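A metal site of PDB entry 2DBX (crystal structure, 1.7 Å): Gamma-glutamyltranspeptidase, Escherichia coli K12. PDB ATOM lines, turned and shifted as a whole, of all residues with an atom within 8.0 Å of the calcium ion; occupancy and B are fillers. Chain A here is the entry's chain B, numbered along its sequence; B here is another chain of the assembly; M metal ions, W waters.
The calcium ion is bound by water W1, O of Ser 182, water W2, OD1 of Asp 185, O of Asp 179 and OD2 of Asp 185.
CA of Pro 180 touches the calcium ion, at 3.96 Å.
Of the 18 residues printed, 4 come within 4 Å of the calcium ion.
OD1 of Asp 179 is in salt-bridge range of NH1 of Arg 181 (2.8 Å).
OG of Ser 182 is in hydrogen-bond range of OG of Ser 162 (2.8 Å).
The side-chain carboxylate of Asp 179 is in hydrogen-bond range of the backbone NH of Thr 163 (2.8 Å).
The side-chain carboxylate (OD2) of Asp 185 lies close to the side-chain amide nitrogen (NE2) of Gln 164 (3.2 Å).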
ATOM      1  N   THR A 119      -6.727  21.180  16.849  1.00  0.00           N
ATOM      2  CA  THR A 119      -7.925  21.910  16.460  1.00  0.00           C
ATOM      3  C   THR A 119      -9.222  21.319  17.003  1.00  0.00           C
ATOM      4  O   THR A 119     -10.115  22.046  17.438  1.00  0.00           O
ATOM      5  CB  THR A 119      -8.017  21.968  14.913  1.00  0.00           C
ATOM      6  OG1 THR A 119      -6.928  22.747  14.405  1.00  0.00           O
ATOM      7  CG2 THR A 119      -9.338  22.572  14.469  1.00  0.00           C
ATOM      8  N   ASN A 120      -9.309  19.990  16.992  1.00  0.00           N
ATOM      9  CA  ASN A 120     -10.512  19.299  17.454  1.00  0.00           C
ATOM     10  C   ASN A 120     -10.600  19.087  18.957  1.00  0.00           C
ATOM     11  O   ASN A 120     -11.626  18.648  19.464  1.00  0.00           O
ATOM     12  CB  ASN A 120     -10.638  17.963  16.716  1.00  0.00           C
ATOM     13  CG  ASN A 120     -11.055  18.133  15.261  1.00  0.00           C
ATOM     14  OD1 ASN A 120     -12.245  18.145  14.941  1.00  0.00           O
ATOM     15  ND2 ASN A 120     -10.070  18.290  14.375  1.00  0.00           N
ATOM     16  N   SER A 162     -12.927  29.488  16.164  1.00  0.00           N
ATOM     17  CA  SER A 162     -12.903  28.894  14.834  1.00  0.00           C
ATOM     18  C   SER A 162     -11.475  29.051  14.319  1.00  0.00           C
ATOM     19  O   SER A 162     -11.160  29.985  13.581  1.00  0.00           O
ATOM     20  CB  SER A 162     -13.878  29.608  13.897  1.00  0.00           C
ATOM     21  OG  SER A 162     -13.801  29.082  12.575  1.00  0.00           O
ATOM     22  N   THR A 163     -10.617  28.142  14.751  1.00  0.00           N
ATOM     23  CA  THR A 163      -9.225  28.183  14.315  1.00  0.00           C
ATOM     24  C   THR A 163      -9.123  27.682  12.887  1.00  0.00           C
ATOM     25  O   THR A 163      -9.826  26.748  12.484  1.00  0.00           O
ATOM     26  CB  THR A 163      -8.319  27.295  15.203  1.00  0.00           C
ATOM     27  OG1 THR A 163      -8.838  25.958  15.226  1.00  0.00           O
ATOM     28  CG2 THR A 163      -8.276  27.839  16.622  1.00  0.00           C
ATOM     29  N   GLN A 164      -8.263  28.314  12.107  1.00  0.00           N
ATOM     30  CA  GLN A 164      -8.030  27.940  10.710  1.00  0.00           C
ATOM     31  C   GLN A 164      -6.503  27.970  10.679  1.00  0.00           C
ATOM     32  O   GLN A 164      -5.900  29.038  10.577  1.00  0.00           O
ATOM     33  CB  GLN A 164      -8.640  28.986   9.774  1.00  0.00           C
ATOM     34  CG  GLN A 164     -10.172  29.152   9.903  1.00  0.00           C
ATOM     35  CD  GLN A 164     -10.949  27.877   9.591  1.00  0.00           C
ATOM     36  OE1 GLN A 164     -10.501  27.039   8.798  1.00  0.00           O
ATOM     37  NE2 GLN A 164     -12.128  27.731  10.187  1.00  0.00           N
ATOM     38  N   ALA A 177      -5.850  22.424   9.044  1.00  0.00           N
ATOM     39  CA  ALA A 177      -7.070  22.024   9.709  1.00  0.00           C
ATOM     40  C   ALA A 177      -8.042  23.165   9.913  1.00  0.00           C
ATOM     41  O   ALA A 177      -7.650  24.264  10.322  1.00  0.00           O
ATOM     42  CB  ALA A 177      -6.754  21.384  11.053  1.00  0.00           C
ATOM     43  N   SER A 178      -9.307  22.893   9.623  1.00  0.00           N
ATOM     44  CA  SER A 178     -10.372  23.864   9.813  1.00  0.00           C
ATOM     45  C   SER A 178     -11.107  23.400  11.067  1.00  0.00           C
ATOM     46  O   SER A 178     -11.182  22.209  11.356  1.00  0.00           O
ATOM     47  CB  SER A 178     -11.323  23.891   8.609  1.00  0.00           C
ATOM     48  OG  SER A 178     -10.777  24.685   7.572  1.00  0.00           O
ATOM     49  N   ASP A 179     -11.651  24.354  11.804  1.00  0.00           N
ATOM     50  CA  ASP A 179     -12.350  24.074  13.065  1.00  0.00           C
ATOM     51  C   ASP A 179     -13.666  23.310  12.935  1.00  0.00           C
ATOM     52  O   ASP A 179     -14.507  23.630  12.101  1.00  0.00           O
ATOM     53  CB  ASP A 179     -12.602  25.401  13.759  1.00  0.00           C
ATOM     54  CG  ASP A 179     -12.715  25.276  15.260  1.00  0.00           C
ATOM     55  OD1 ASP A 179     -13.449  24.386  15.728  1.00  0.00           O
ATOM     56  OD2 ASP A 179     -12.065  26.073  15.963  1.00  0.00           O
ATOM     57  N   PRO A 180     -13.876  22.272  13.771  1.00  0.00           N
ATOM     58  CA  PRO A 180     -15.153  21.552  13.665  1.00  0.00           C
ATOM     59  C   PRO A 180     -16.325  22.430  14.119  1.00  0.00           C
ATOM     60  O   PRO A 180     -17.480  22.177  13.762  1.00  0.00           O
ATOM     61  CB  PRO A 180     -14.949  20.345  14.594  1.00  0.00           C
ATOM     62  CG  PRO A 180     -13.988  20.865  15.617  1.00  0.00           C
ATOM     63  CD  PRO A 180     -13.002  21.627  14.760  1.00  0.00           C
ATOM     64  N   ARG A 181     -16.025  23.468  14.894  1.00  0.00           N
ATOM     65  CA  ARG A 181     -17.053  24.361  15.411  1.00  0.00           C
ATOM     66  C   ARG A 181     -17.741  25.226  14.362  1.00  0.00           C
ATOM     67  O   ARG A 181     -18.841  25.726  14.586  1.00  0.00           O
ATOM     68  CB  ARG A 181     -16.447  25.257  16.496  1.00  0.00           C
ATOM     69  CG  ARG A 181     -15.839  24.457  17.628  1.00  0.00           C
ATOM     70  CD  ARG A 181     -14.951  25.315  18.506  1.00  0.00           C
ATOM     71  NE  ARG A 181     -14.340  24.543  19.582  1.00  0.00           N
ATOM     72  CZ  ARG A 181     -13.378  23.641  19.429  1.00  0.00           C
ATOM     73  NH1 ARG A 181     -12.881  23.372  18.228  1.00  0.00           N
ATOM     74  NH2 ARG A 181     -12.903  23.002  20.489  1.00  0.00           N
ATOM     75  N   SER A 182     -17.103  25.401  13.208  1.00  0.00           N
ATOM     76  CA  SER A 182     -17.702  26.201  12.147  1.00  0.00           C
ATOM     77  C   SER A 182     -17.986  25.348  10.911  1.00  0.00           C
ATOM     78  O   SER A 182     -17.100  24.673  10.408  1.00  0.00           O
ATOM     79  CB  SER A 182     -16.790  27.384  11.801  1.00  0.00           C
ATOM     80  OG  SER A 182     -15.429  26.990  11.758  1.00  0.00           O
ATOM     81  N   VAL A 183     -19.215  25.381  10.405  1.00  0.00           N
ATOM     82  CA  VAL A 183     -19.527  24.589   9.224  1.00  0.00           C
ATOM     83  C   VAL A 183     -19.298  25.382   7.941  1.00  0.00           C
ATOM     84  O   VAL A 183     -19.245  26.606   7.973  1.00  0.00           O
ATOM     85  CB  VAL A 183     -20.992  24.084   9.238  1.00  0.00           C
ATOM     86  CG1 VAL A 183     -21.220  23.215  10.456  1.00  0.00           C
ATOM     87  CG2 VAL A 183     -21.945  25.271   9.216  1.00  0.00           C
ATOM     88  N   ASP A 184     -19.156  24.670   6.836  1.00  0.00           N
ATOM     89  CA  ASP A 184     -18.940  25.258   5.509  1.00  0.00           C
ATOM     90  C   ASP A 184     -17.589  25.953   5.320  1.00  0.00           C
ATOM     91  O   ASP A 184     -17.402  26.717   4.364  1.00  0.00           O
ATOM     92  CB  ASP A 184     -20.071  26.232   5.162  1.00  0.00           C
ATOM     93  CG  ASP A 184     -21.401  25.528   5.011  1.00  0.00           C
ATOM     94  OD1 ASP A 184     -21.436  24.442   4.382  1.00  0.00           O
ATOM     95  OD2 ASP A 184     -22.425  26.057   5.504  1.00  0.00           O
ATOM     96  N   ASP A 185     -16.646  25.679   6.214  1.00  0.00           N
ATOM     97  CA  ASP A 185     -15.311  26.252   6.105  1.00  0.00           C
ATOM     98  C   ASP A 185     -14.446  25.262   5.326  1.00  0.00           C
ATOM     99  O   ASP A 185     -14.905  24.173   4.970  1.00  0.00           O
ATOM    100  CB  ASP A 185     -14.710  26.511   7.487  1.00  0.00           C
ATOM    101  CG  ASP A 185     -14.712  25.273   8.360  1.00  0.00           C
ATOM    102  OD1 ASP A 185     -15.235  24.240   7.907  1.00  0.00           O
ATOM    103  OD2 ASP A 185     -14.200  25.340   9.492  1.00  0.00           O
ATOM    104  N   LEU A 186     -13.199  25.631   5.053  1.00  0.00           N
ATOM    105  CA  LEU A 186     -12.335  24.750   4.298  1.00  0.00           C
ATOM    106  C   LEU A 186     -10.854  25.081   4.346  1.00  0.00           C
ATOM    107  O   LEU A 186     -10.460  26.250   4.367  1.00  0.00           O
ATOM    108  CB  LEU A 186     -12.776  24.743   2.819  1.00  0.00           C
ATOM    109  CG  LEU A 186     -12.013  23.853   1.832  1.00  0.00           C
ATOM    110  CD1 LEU A 186     -12.317  22.391   2.123  1.00  0.00           C
ATOM    111  CD2 LEU A 186     -12.427  24.207   0.399  1.00  0.00           C
ATOM    112  N   THR A 187     -10.052  24.031   4.378  1.00  0.00           N
ATOM    113  CA  THR A 187      -8.603  24.150   4.329  1.00  0.00           C
ATOM    114  C   THR A 187      -8.285  23.316   3.085  1.00  0.00           C
ATOM    115  O   THR A 187      -8.681  22.152   3.000  1.00  0.00           O
ATOM    116  CB  THR A 187      -7.916  23.548   5.575  1.00  0.00           C
ATOM    117  OG1 THR A 187      -8.218  24.361   6.711  1.00  0.00           O
ATOM    118  CG2 THR A 187      -6.403  23.504   5.381  1.00  0.00           C
ATOM    119  N   SER B  29      -9.569  28.809   5.722  1.00  0.00           N
ATOM    120  CA  SER B  29     -10.492  29.898   6.049  1.00  0.00           C
ATOM    121  C   SER B  29     -11.862  29.367   6.453  1.00  0.00           C
ATOM    122  O   SER B  29     -12.152  28.181   6.305  1.00  0.00           O
ATOM    123  CB  SER B  29     -10.650  30.885   4.879  1.00  0.00           C
ATOM    124  OG  SER B  29     -11.715  30.517   4.032  1.00  0.00           O
ATOM    125  N   VAL B  30     -12.700  30.253   6.977  1.00  0.00           N
ATOM    126  CA  VAL B  30     -14.030  29.901   7.453  1.00  0.00           C
ATOM    127  C   VAL B  30     -15.033  29.657   6.325  1.00  0.00           C
ATOM    128  O   VAL B  30     -16.150  29.217   6.569  1.00  0.00           O
ATOM    129  CB  VAL B  30     -14.593  31.023   8.354  1.00  0.00           C
ATOM    130  CG1 VAL B  30     -15.022  32.207   7.504  1.00  0.00           C
ATOM    131  CG2 VAL B  30     -15.742  30.491   9.203  1.00  0.00           C
HETATM  132 CA    CA M   1     -15.550  22.936   9.976  1.00  0.00          CA
HETATM  133  O   HOH W   1     -16.850  21.718   8.443  1.00  0.00           O
HETATM  134  O   HOH W   2     -13.603  21.659   9.461  1.00  0.00           O
